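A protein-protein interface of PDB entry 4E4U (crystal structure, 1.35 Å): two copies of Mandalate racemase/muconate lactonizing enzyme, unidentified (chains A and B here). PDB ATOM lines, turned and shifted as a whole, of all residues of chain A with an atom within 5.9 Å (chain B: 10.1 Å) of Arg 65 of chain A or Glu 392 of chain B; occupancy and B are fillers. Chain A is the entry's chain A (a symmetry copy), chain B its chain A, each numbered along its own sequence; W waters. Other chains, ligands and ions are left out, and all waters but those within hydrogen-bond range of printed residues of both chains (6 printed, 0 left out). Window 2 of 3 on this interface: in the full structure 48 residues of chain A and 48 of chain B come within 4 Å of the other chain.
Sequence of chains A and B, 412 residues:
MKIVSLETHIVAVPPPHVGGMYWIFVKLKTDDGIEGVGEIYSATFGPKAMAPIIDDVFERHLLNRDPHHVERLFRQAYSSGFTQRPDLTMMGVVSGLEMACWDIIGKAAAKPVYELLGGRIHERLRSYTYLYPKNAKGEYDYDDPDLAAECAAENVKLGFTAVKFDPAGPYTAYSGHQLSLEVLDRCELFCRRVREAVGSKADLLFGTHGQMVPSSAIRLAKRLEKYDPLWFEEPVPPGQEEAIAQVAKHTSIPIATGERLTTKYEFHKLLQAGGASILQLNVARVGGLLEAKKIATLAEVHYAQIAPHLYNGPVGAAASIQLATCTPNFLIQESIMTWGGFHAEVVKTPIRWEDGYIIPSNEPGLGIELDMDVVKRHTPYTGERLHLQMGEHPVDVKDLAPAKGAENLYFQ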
ATOM      1  N   MET A   1     -12.475  16.292   6.113  1.00  0.00           N
ATOM      2  CA  MET A   1     -12.355  17.643   5.590  1.00  0.00           C
ATOM      3  C   MET A   1     -12.136  18.664   6.695  1.00  0.00           C
ATOM      4  O   MET A   1     -12.894  18.695   7.658  1.00  0.00           O
ATOM      5  CB  MET A   1     -13.633  18.035   4.887  1.00  0.00           C
ATOM      6  CG  MET A   1     -13.551  19.432   4.389  1.00  0.00           C
ATOM      7  SD  MET A   1     -12.416  19.329   3.045  1.00  0.00           S
ATOM      8  CE  MET A   1     -13.522  19.972   1.792  1.00  0.00           C
ATOM      9  N   LYS A   2     -11.132  19.523   6.541  1.00  0.00           N
ATOM     10  CA  LYS A   2     -10.894  20.551   7.549  1.00  0.00           C
ATOM     11  C   LYS A   2     -10.320  21.848   6.981  1.00  0.00           C
ATOM     12  O   LYS A   2      -9.671  21.850   5.939  1.00  0.00           O
ATOM     13  CB  LYS A   2      -9.984  20.016   8.657  1.00  0.00           C
ATOM     14  CG  LYS A   2      -8.538  19.854   8.246  1.00  0.00           C
ATOM     15  CD  LYS A   2      -7.727  19.193   9.356  1.00  0.00           C
ATOM     16  CE  LYS A   2      -6.250  19.100   8.987  1.00  0.00           C
ATOM     17  NZ  LYS A   2      -5.407  18.662  10.133  1.00  0.00           N
ATOM     18  N   ILE A   3     -10.570  22.952   7.680  1.00  0.00           N
ATOM     19  CA  ILE A   3     -10.035  24.250   7.280  1.00  0.00           C
ATOM     20  C   ILE A   3      -8.582  24.338   7.708  1.00  0.00           C
ATOM     21  O   ILE A   3      -8.264  24.124   8.880  1.00  0.00           O
ATOM     22  CB  ILE A   3     -10.801  25.406   7.947  1.00  0.00           C
ATOM     23  CG1 ILE A   3     -12.288  25.346   7.599  1.00  0.00           C
ATOM     24  CG2 ILE A   3     -10.198  26.745   7.541  1.00  0.00           C
ATOM     25  CD1 ILE A   3     -12.572  25.473   6.115  1.00  0.00           C
ATOM     26  N   ARG A  60      -7.915  30.324  17.121  1.00  0.00           N
ATOM     27  CA  ARG A  60      -8.485  29.713  18.317  1.00  0.00           C
ATOM     28  C   ARG A  60      -9.689  28.841  18.028  1.00  0.00           C
ATOM     29  O   ARG A  60      -9.874  27.816  18.681  1.00  0.00           O
ATOM     30  CB  ARG A  60      -8.881  30.779  19.351  1.00  0.00           C
ATOM     31  CG  ARG A  60      -7.716  31.555  19.897  1.00  0.00           C
ATOM     32  CD  ARG A  60      -8.169  32.621  20.883  1.00  0.00           C
ATOM     33  NE  ARG A  60      -7.073  33.556  21.075  1.00  0.00           N
ATOM     34  CZ  ARG A  60      -6.030  33.327  21.861  1.00  0.00           C
ATOM     35  NH1 ARG A  60      -5.962  32.207  22.577  1.00  0.00           N
ATOM     36  NH2 ARG A  60      -5.061  34.226  21.945  1.00  0.00           N
ATOM     37  N   HIS A  61     -10.516  29.244  17.064  1.00  0.00           N
ATOM     38  CA  HIS A  61     -11.861  28.683  16.973  1.00  0.00           C
ATOM     39  C   HIS A  61     -12.205  27.977  15.662  1.00  0.00           C
ATOM     40  O   HIS A  61     -13.268  27.376  15.573  1.00  0.00           O
ATOM     41  CB  HIS A  61     -12.916  29.764  17.274  1.00  0.00           C
ATOM     42  CG  HIS A  61     -12.703  30.461  18.578  1.00  0.00           C
ATOM     43  ND1 HIS A  61     -12.697  29.809  19.793  1.00  0.00           N
ATOM     44  CD2 HIS A  61     -12.491  31.779  18.859  1.00  0.00           C
ATOM     45  CE1 HIS A  61     -12.487  30.675  20.758  1.00  0.00           C
ATOM     46  NE2 HIS A  61     -12.361  31.878  20.229  1.00  0.00           N
ATOM     47  N   LEU A  62     -11.333  28.036  14.652  1.00  0.00           N
ATOM     48  CA  LEU A  62     -11.672  27.428  13.357  1.00  0.00           C
ATOM     49  C   LEU A  62     -10.547  26.613  12.718  1.00  0.00           C
ATOM     50  O   LEU A  62     -10.812  25.609  12.060  1.00  0.00           O
ATOM     51  CB  LEU A  62     -12.182  28.476  12.360  1.00  0.00           C
ATOM     52  CG  LEU A  62     -12.710  27.939  11.020  1.00  0.00           C
ATOM     53  CD1 LEU A  62     -13.789  26.868  11.230  1.00  0.00           C
ATOM     54  CD2 LEU A  62     -13.237  29.074  10.160  1.00  0.00           C
ATOM     55  N   LEU A  63      -9.302  27.047  12.890  1.00  0.00           N
ATOM     56  CA  LEU A  63      -8.173  26.327  12.310  1.00  0.00           C
ATOM     57  C   LEU A  63      -8.233  24.838  12.651  1.00  0.00           C
ATOM     58  O   LEU A  63      -8.411  24.465  13.815  1.00  0.00           O
ATOM     59  CB  LEU A  63      -6.849  26.927  12.782  1.00  0.00           C
ATOM     60  CG  LEU A  63      -5.580  26.187  12.340  1.00  0.00           C
ATOM     61  CD1 LEU A  63      -5.421  26.195  10.816  1.00  0.00           C
ATOM     62  CD2 LEU A  63      -4.343  26.772  13.005  1.00  0.00           C
ATOM     63  N   ASN A  64      -8.132  24.008  11.611  1.00  0.00           N
ATOM     64  CA  ASN A  64      -8.152  22.548  11.706  1.00  0.00           C
ATOM     65  C   ASN A  64      -9.493  21.916  12.059  1.00  0.00           C
ATOM     66  O   ASN A  64      -9.553  20.733  12.400  1.00  0.00           O
ATOM     67  CB  ASN A  64      -7.022  22.032  12.603  1.00  0.00           C
ATOM     68  CG  ASN A  64      -5.665  22.246  11.984  1.00  0.00           C
ATOM     69  OD1 ASN A  64      -5.498  22.093  10.774  1.00  0.00           O
ATOM     70  ND2 ASN A  64      -4.694  22.626  12.797  1.00  0.00           N
ATOM     71  N   ARG A  65     -10.566  22.691  11.938  1.00  0.00           N
ATOM     72  CA  ARG A  65     -11.917  22.198  12.207  1.00  0.00           C
ATOM     73  C   ARG A  65     -12.678  21.915  10.909  1.00  0.00           C
ATOM     74  O   ARG A  65     -12.367  22.469   9.851  1.00  0.00           O
ATOM     75  CB  ARG A  65     -12.705  23.203  13.057  1.00  0.00           C
ATOM     76  CG  ARG A  65     -12.092  23.487  14.418  1.00  0.00           C
ATOM     77  CD  ARG A  65     -12.130  22.276  15.337  1.00  0.00           C
ATOM     78  NE  ARG A  65     -11.435  22.566  16.587  1.00  0.00           N
ATOM     79  CZ  ARG A  65     -11.248  21.690  17.566  1.00  0.00           C
ATOM     80  NH1 ARG A  65     -11.715  20.455  17.458  1.00  0.00           N
ATOM     81  NH2 ARG A  65     -10.592  22.054  18.661  1.00  0.00           N
ATOM     82  N   ASP A  66     -13.687  21.058  10.998  1.00  0.00           N
ATOM     83  CA  ASP A  66     -14.523  20.720   9.851  1.00  0.00           C
ATOM     84  C   ASP A  66     -15.440  21.902   9.518  1.00  0.00           C
ATOM     85  O   ASP A  66     -16.167  22.377  10.388  1.00  0.00           O
ATOM     86  CB  ASP A  66     -15.360  19.489  10.215  1.00  0.00           C
ATOM     87  CG  ASP A  66     -16.071  18.872   9.028  1.00  0.00           C
ATOM     88  OD1 ASP A  66     -16.540  19.614   8.139  1.00  0.00           O
ATOM     89  OD2 ASP A  66     -16.171  17.625   8.995  1.00  0.00           O
ATOM     90  N   PRO A  67     -15.431  22.371   8.256  1.00  0.00           N
ATOM     91  CA  PRO A  67     -16.312  23.495   7.900  1.00  0.00           C
ATOM     92  C   PRO A  67     -17.804  23.209   8.089  1.00  0.00           C
ATOM     93  O   PRO A  67     -18.584  24.156   8.207  1.00  0.00           O
ATOM     94  CB  PRO A  67     -16.008  23.726   6.413  1.00  0.00           C
ATOM     95  CG  PRO A  67     -15.450  22.428   5.930  1.00  0.00           C
ATOM     96  CD  PRO A  67     -14.656  21.898   7.093  1.00  0.00           C
ATOM     97  N   HIS A  69     -19.158  22.158  10.667  1.00  0.00           N
ATOM     98  CA  HIS A  69     -19.511  22.278  12.075  1.00  0.00           C
ATOM     99  C   HIS A  69     -19.772  23.727  12.478  1.00  0.00           C
ATOM    100  O   HIS A  69     -19.062  24.305  13.309  1.00  0.00           O
ATOM    101  CB  HIS A  69     -18.448  21.588  12.935  1.00  0.00           C
ATOM    102  CG  HIS A  69     -18.338  20.121  12.654  1.00  0.00           C
ATOM    103  ND1 HIS A  69     -17.369  19.322  13.208  1.00  0.00           N
ATOM    104  CD2 HIS A  69     -19.078  19.323  11.846  1.00  0.00           C
ATOM    105  CE1 HIS A  69     -17.519  18.085  12.767  1.00  0.00           C
ATOM    106  NE2 HIS A  69     -18.549  18.057  11.938  1.00  0.00           N
ATOM    107  N   ARG A  72     -20.856  24.456  16.133  1.00  0.00           N
ATOM    108  CA  ARG A  72     -19.646  24.444  16.943  1.00  0.00           C
ATOM    109  C   ARG A  72     -18.910  25.770  16.808  1.00  0.00           C
ATOM    110  O   ARG A  72     -18.534  26.391  17.811  1.00  0.00           O
ATOM    111  CB  ARG A  72     -18.740  23.295  16.494  1.00  0.00           C
ATOM    112  CG  ARG A  72     -17.413  23.192  17.232  1.00  0.00           C
ATOM    113  CD  ARG A  72     -16.317  22.634  16.299  1.00  0.00           C
ATOM    114  NE  ARG A  72     -15.998  23.615  15.261  1.00  0.00           N
ATOM    115  CZ  ARG A  72     -15.198  24.661  15.447  1.00  0.00           C
ATOM    116  NH1 ARG A  72     -14.598  24.847  16.620  1.00  0.00           N
ATOM    117  NH2 ARG A  72     -14.986  25.515  14.456  1.00  0.00           N
ATOM    118  N   GLN A  76     -18.290  28.340  19.898  1.00  0.00           N
ATOM    119  CA  GLN A  76     -16.935  28.623  20.365  1.00  0.00           C
ATOM    120  C   GLN A  76     -16.641  30.120  20.317  1.00  0.00           C
ATOM    121  O   GLN A  76     -16.079  30.681  21.255  1.00  0.00           O
ATOM    122  CB  GLN A  76     -15.883  27.860  19.548  1.00  0.00           C
ATOM    123  CG  GLN A  76     -16.011  26.341  19.583  1.00  0.00           C
ATOM    124  CD  GLN A  76     -15.902  25.744  20.972  1.00  0.00           C
ATOM    125  OE1 GLN A  76     -15.080  26.167  21.790  1.00  0.00           O
ATOM    126  NE2 GLN A  76     -16.712  24.721  21.236  1.00  0.00           N
ATOM    127  N   PRO B 170     -17.608  21.925  34.973  1.00  0.00           N
ATOM    128  CA  PRO B 170     -17.169  22.787  33.873  1.00  0.00           C
ATOM    129  C   PRO B 170     -18.264  23.697  33.332  1.00  0.00           C
ATOM    130  O   PRO B 170     -19.450  23.336  33.278  1.00  0.00           O
ATOM    131  CB  PRO B 170     -16.779  21.784  32.783  1.00  0.00           C
ATOM    132  CG  PRO B 170     -16.426  20.533  33.531  1.00  0.00           C
ATOM    133  CD  PRO B 170     -17.413  20.498  34.666  1.00  0.00           C
ATOM    134  N   TYR B 171     -17.848  24.895  32.942  1.00  0.00           N
ATOM    135  CA  TYR B 171     -18.671  25.768  32.127  1.00  0.00           C
ATOM    136  C   TYR B 171     -18.104  25.701  30.716  1.00  0.00           C
ATOM    137  O   TYR B 171     -16.897  25.831  30.520  1.00  0.00           O
ATOM    138  CB  TYR B 171     -18.671  27.202  32.667  1.00  0.00           C
ATOM    139  CG  TYR B 171     -17.328  27.722  33.136  1.00  0.00           C
ATOM    140  CD1 TYR B 171     -16.876  27.471  34.425  1.00  0.00           C
ATOM    141  CD2 TYR B 171     -16.540  28.513  32.311  1.00  0.00           C
ATOM    142  CE1 TYR B 171     -15.665  27.964  34.867  1.00  0.00           C
ATOM    143  CE2 TYR B 171     -15.328  29.011  32.744  1.00  0.00           C
ATOM    144  CZ  TYR B 171     -14.894  28.733  34.026  1.00  0.00           C
ATOM    145  OH  TYR B 171     -13.688  29.222  34.476  1.00  0.00           O
ATOM    146  N   THR B 172     -18.967  25.464  29.736  1.00  0.00           N
ATOM    147  CA  THR B 172     -18.493  25.146  28.395  1.00  0.00           C
ATOM    148  C   THR B 172     -19.135  26.049  27.364  1.00  0.00           C
ATOM    149  O   THR B 172     -20.067  26.797  27.670  1.00  0.00           O
ATOM    150  CB  THR B 172     -18.808  23.687  27.989  1.00  0.00           C
ATOM    151  OG1 THR B 172     -20.151  23.604  27.494  1.00  0.00           O
ATOM    152  CG2 THR B 172     -18.612  22.724  29.161  1.00  0.00           C
ATOM    153  N   ALA B 173     -18.653  25.944  26.129  1.00  0.00           N
ATOM    154  CA  ALA B 173     -19.200  26.695  25.009  1.00  0.00           C
ATOM    155  C   ALA B 173     -20.666  26.366  24.744  1.00  0.00           C
ATOM    156  O   ALA B 173     -21.339  27.115  24.052  1.00  0.00           O
ATOM    157  CB  ALA B 173     -18.375  26.450  23.750  1.00  0.00           C
ATOM    158  N   TYR B 174     -21.155  25.255  25.295  1.00  0.00           N
ATOM    159  CA  TYR B 174     -22.528  24.809  25.053  1.00  0.00           C
ATOM    160  C   TYR B 174     -23.427  24.992  26.264  1.00  0.00           C
ATOM    161  O   TYR B 174     -24.600  24.624  26.228  1.00  0.00           O
ATOM    162  CB  TYR B 174     -22.535  23.347  24.582  1.00  0.00           C
ATOM    163  CG  TYR B 174     -21.669  23.179  23.358  1.00  0.00           C
ATOM    164  CD1 TYR B 174     -22.154  23.489  22.094  1.00  0.00           C
ATOM    165  CD2 TYR B 174     -20.353  22.747  23.468  1.00  0.00           C
ATOM    166  CE1 TYR B 174     -21.350  23.372  20.970  1.00  0.00           C
ATOM    167  CE2 TYR B 174     -19.542  22.621  22.351  1.00  0.00           C
ATOM    168  CZ  TYR B 174     -20.044  22.924  21.104  1.00  0.00           C
ATOM    169  OH  TYR B 174     -19.243  22.805  19.988  1.00  0.00           O
ATOM    170  N   SER B 175     -22.889  25.570  27.334  1.00  0.00           N
ATOM    171  CA  SER B 175     -23.720  25.939  28.473  1.00  0.00           C
ATOM    172  C   SER B 175     -24.802  26.922  27.999  1.00  0.00           C
ATOM    173  O   SER B 175     -24.580  27.670  27.037  1.00  0.00           O
ATOM    174  CB  SER B 175     -22.856  26.540  29.586  1.00  0.00           C
ATOM    175  OG  SER B 175     -21.999  25.551  30.136  1.00  0.00           O
ATOM    176  N   ARG B 385      -3.074  30.832  25.858  1.00  0.00           N
ATOM    177  CA  ARG B 385      -4.448  30.951  26.337  1.00  0.00           C
ATOM    178  C   ARG B 385      -4.948  32.384  26.462  1.00  0.00           C
ATOM    179  O   ARG B 385      -4.160  33.326  26.592  1.00  0.00           O
ATOM    180  CB  ARG B 385      -4.600  30.250  27.690  1.00  0.00           C
ATOM    181  CG  ARG B 385      -4.444  28.737  27.635  1.00  0.00           C
ATOM    182  CD  ARG B 385      -4.632  28.117  29.014  1.00  0.00           C
ATOM    183  NE  ARG B 385      -5.986  28.293  29.533  1.00  0.00           N
ATOM    184  CZ  ARG B 385      -6.951  27.383  29.435  1.00  0.00           C
ATOM    185  NH1 ARG B 385      -6.718  26.225  28.829  1.00  0.00           N
ATOM    186  NH2 ARG B 385      -8.151  27.630  29.942  1.00  0.00           N
ATOM    187  N   GLN B 389     -10.991  31.003  29.808  1.00  0.00           N
ATOM    188  CA  GLN B 389     -11.597  30.287  28.684  1.00  0.00           C
ATOM    189  C   GLN B 389     -12.746  29.407  29.150  1.00  0.00           C
ATOM    190  O   GLN B 389     -12.823  29.045  30.331  1.00  0.00           O
ATOM    191  CB  GLN B 389     -10.555  29.421  27.959  1.00  0.00           C
ATOM    192  CG  GLN B 389      -9.436  30.238  27.343  1.00  0.00           C
ATOM    193  CD  GLN B 389      -8.439  29.450  26.511  1.00  0.00           C
ATOM    194  OE1 GLN B 389      -7.510  30.036  25.952  1.00  0.00           O
ATOM    195  NE2 GLN B 389      -8.614  28.131  26.423  1.00  0.00           N
ATOM    196  N   MET B 390     -13.647  29.076  28.228  1.00  0.00           N
ATOM    197  CA  MET B 390     -14.696  28.100  28.511  1.00  0.00           C
ATOM    198  C   MET B 390     -14.317  26.750  27.927  1.00  0.00           C
ATOM    199  O   MET B 390     -13.548  26.678  26.967  1.00  0.00           O
ATOM    200  CB  MET B 390     -16.047  28.568  27.962  1.00  0.00           C
ATOM    201  CG  MET B 390     -16.401  29.973  28.417  1.00  0.00           C
ATOM    202  SD  MET B 390     -18.100  30.458  28.147  1.00  0.00           S
ATOM    203  CE  MET B 390     -18.944  29.525  29.422  1.00  0.00           C
ATOM    204  N   GLY B 391     -14.849  25.682  28.512  1.00  0.00           N
ATOM    205  CA  GLY B 391     -14.598  24.340  28.020  1.00  0.00           C
ATOM    206  C   GLY B 391     -15.008  24.193  26.569  1.00  0.00           C
ATOM    207  O   GLY B 391     -16.012  24.757  26.136  1.00  0.00           O
ATOM    208  N   GLU B 392     -14.235  23.429  25.810  1.00  0.00           N
ATOM    209  CA  GLU B 392     -14.509  23.289  24.388  1.00  0.00           C
ATOM    210  C   GLU B 392     -15.661  22.324  24.079  1.00  0.00           C
ATOM    211  O   GLU B 392     -16.400  22.524  23.112  1.00  0.00           O
ATOM    212  CB  GLU B 392     -13.245  22.852  23.651  1.00  0.00           C
ATOM    213  CG  GLU B 392     -13.426  22.830  22.156  1.00  0.00           C
ATOM    214  CD  GLU B 392     -12.157  22.503  21.413  1.00  0.00           C
ATOM    215  OE1 GLU B 392     -11.184  22.043  22.057  1.00  0.00           O
ATOM    216  OE2 GLU B 392     -12.139  22.712  20.181  1.00  0.00           O
ATOM    217  N   HIS B 393     -15.825  21.288  24.896  1.00  0.00           N
ATOM    218  CA  HIS B 393     -16.814  20.253  24.610  1.00  0.00           C
ATOM    219  C   HIS B 393     -17.978  20.283  25.587  1.00  0.00           C
ATOM    220  O   HIS B 393     -17.823  20.734  26.720  1.00  0.00           O
ATOM    221  CB  HIS B 393     -16.156  18.873  24.646  1.00  0.00           C
ATOM    222  CG  HIS B 393     -14.934  18.766  23.789  1.00  0.00           C
ATOM    223  ND1 HIS B 393     -14.996  18.671  22.417  1.00  0.00           N
ATOM    224  CD2 HIS B 393     -13.621  18.747  24.113  1.00  0.00           C
ATOM    225  CE1 HIS B 393     -13.767  18.593  21.931  1.00  0.00           C
ATOM    226  NE2 HIS B 393     -12.916  18.638  22.938  1.00  0.00           N
ATOM    227  N   PRO B 394     -19.156  19.796  25.156  1.00  0.00           N
ATOM    228  CA  PRO B 394     -20.282  19.745  26.091  1.00  0.00           C
ATOM    229  C   PRO B 394     -19.945  18.831  27.259  1.00  0.00           C
ATOM    230  O   PRO B 394     -19.210  17.854  27.090  1.00  0.00           O
ATOM    231  CB  PRO B 394     -21.404  19.109  25.259  1.00  0.00           C
ATOM    232  CG  PRO B 394     -21.025  19.339  23.848  1.00  0.00           C
ATOM    233  CD  PRO B 394     -19.522  19.282  23.825  1.00  0.00           C
ATOM    234  N   VAL B 395     -20.481  19.148  28.433  1.00  0.00           N
ATOM    235  CA  VAL B 395     -20.318  18.301  29.613  1.00  0.00           C
ATOM    236  C   VAL B 395     -21.004  16.948  29.405  1.00  0.00           C
ATOM    237  O   VAL B 395     -22.119  16.887  28.888  1.00  0.00           O
ATOM    238  CB  VAL B 395     -20.891  18.997  30.877  1.00  0.00           C
ATOM    239  CG1 VAL B 395     -21.139  17.994  31.999  1.00  0.00           C
ATOM    240  CG2 VAL B 395     -19.957  20.107  31.344  1.00  0.00           C
ATOM    241  N   ASP B 396     -20.333  15.865  29.787  1.00  0.00           N
ATOM    242  CA  ASP B 396     -20.947  14.546  29.750  1.00  0.00           C
ATOM    243  C   ASP B 396     -21.524  14.304  31.139  1.00  0.00           C
ATOM    244  O   ASP B 396     -20.898  14.660  32.137  1.00  0.00           O
ATOM    245  CB  ASP B 396     -19.897  13.489  29.408  1.00  0.00           C
ATOM    246  CG  ASP B 396     -20.499  12.108  29.171  1.00  0.00           C
ATOM    247  OD1 ASP B 396     -21.172  11.569  30.076  1.00  0.00           O
ATOM    248  OD2 ASP B 396     -20.286  11.562  28.069  1.00  0.00           O
ATOM    249  N   ALA B 403     -14.970  22.884  37.871  1.00  0.00           N
ATOM    250  CA  ALA B 403     -15.110  24.099  37.074  1.00  0.00           C
ATOM    251  C   ALA B 403     -13.745  24.670  36.703  1.00  0.00           C
ATOM    252  O   ALA B 403     -13.566  25.219  35.618  1.00  0.00           O
ATOM    253  CB  ALA B 403     -15.939  25.141  37.829  1.00  0.00           C
HETATM  254  O   HOH W   1     -14.139  26.993  24.190  1.00  0.00           O
HETATM  255  O   HOH W   2     -11.935  25.060  19.682  1.00  0.00           O
HETATM  256  O   HOH W   3      -3.143  34.126  23.968  1.00  0.00           O
HETATM  257  O   HOH W   4     -14.292  23.330  18.963  1.00  0.00           O
HETATM  258  O   HOH W   5      -7.952  30.097  23.287  1.00  0.00           O
HETATM  259  O   HOH W   6     -16.972  21.353  20.467  1.00  0.00           O
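Of the printed residues of chain B, Arg 65 of chain A touches Glu 392. Pro 67 of chain A touches none of the printed residues of chain B. Printed residues of chain B within 4 Å of Arg 72 of chain A: Tyr 174. Of the printed residues of chain B, Gln 76 of chain A touches Ala 173, Tyr 174 and Glu 392. Printed residues of chain A within 4 Å of Ala 173 of chain B: Gln 76. Printed residues of chain A within 4 Å of Tyr 174 of chain B: Arg 72 and Gln 76. Printed residues of chain A within 4 Å of Glu 392 of chain B: Arg 65 and Gln 76. The nearest printed residue of chain B that does not touch Arg 65 of chain A is His 393 of chain B (5.3 Å).
N of Ile 3 of chain A is in hydrogen-bond range of O of Arg 65 of chain A, at 2.9 Å. The guanidinium group (NH2) of Arg 72 of chain A sits at hydrogen-bond distance from the backbone carbonyl oxygen (O) of His 61 of chain A, at 2.8 Å. O of Gly 391 of chain B is in hydrogen-bond range of N of Ala 173 of chain B, 2.9 Å away. The side-chain hydroxyl (OG1) of Thr 172 of chain B sits at hydrogen-bond distance from the backbone NH (N) of Tyr 174 of chain B (2.9 Å).
NE2 of Gln 76 of chain A is in hydrogen-bond range of OH of Tyr 174 of chain B, 3.4 Å away. OE1 of Glu 392 of chain B is in salt-bridge range of NH2 of Arg 65 of chain A. The backbone carbonyl oxygen of Glu 392 of chain B sits at hydrogen-bond distance from the side-chain amide nitrogen of Gln 76 of chain A.
Among the printed residues, merely in contact across the chains: Arg 72 of chain A with Tyr 174 of chain B (3.3 Å) and Gln 76 of chain A with Ala 173 of chain B (3.5 Å).
Along chain B the printed residues that touch a printed residue of chain A span positions 173 to 392. Printed residues of chain A that touch a printed residue of chain B: Arg 65, Arg 72 and Gln 76. Among the printed residues, 5 pairs touch across the chains.
No position is printed for both chains.
Water W2 lies within hydrogen-bond range of the side-chain carboxylate of Glu 392 of chain B (2.4 Å) and the guanidinium group of Arg 65 of chain A (3.4 Å). Water W4 bridges OE2 of Glu 392 of chain B (2.5 Å) and NH1 of Arg 72 of chain A (2.8 Å). Water W5 bridges OE1 of Gln 389 of chain B and NH1 of Arg 60 of chain A. Water W1 lies within hydrogen-bond range of OE1 of Gln 76 of chain A and O of Met 390 of chain B. Water W6 lies within hydrogen-bond range of the side-chain hydroxyl (OH) of Tyr 174 of chain B (2.7 Å), the backbone carbonyl oxygen (O) of Glu 392 of chain B (2.9 Å) and the side-chain amide nitrogen (NE2) of Gln 76 of chain A (3.5 Å). Water W3 bridges the guanidinium group of Arg 60 of chain A (2.8 Å) and the backbone carbonyl oxygen of Arg 385 of chain B (2.9 Å).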
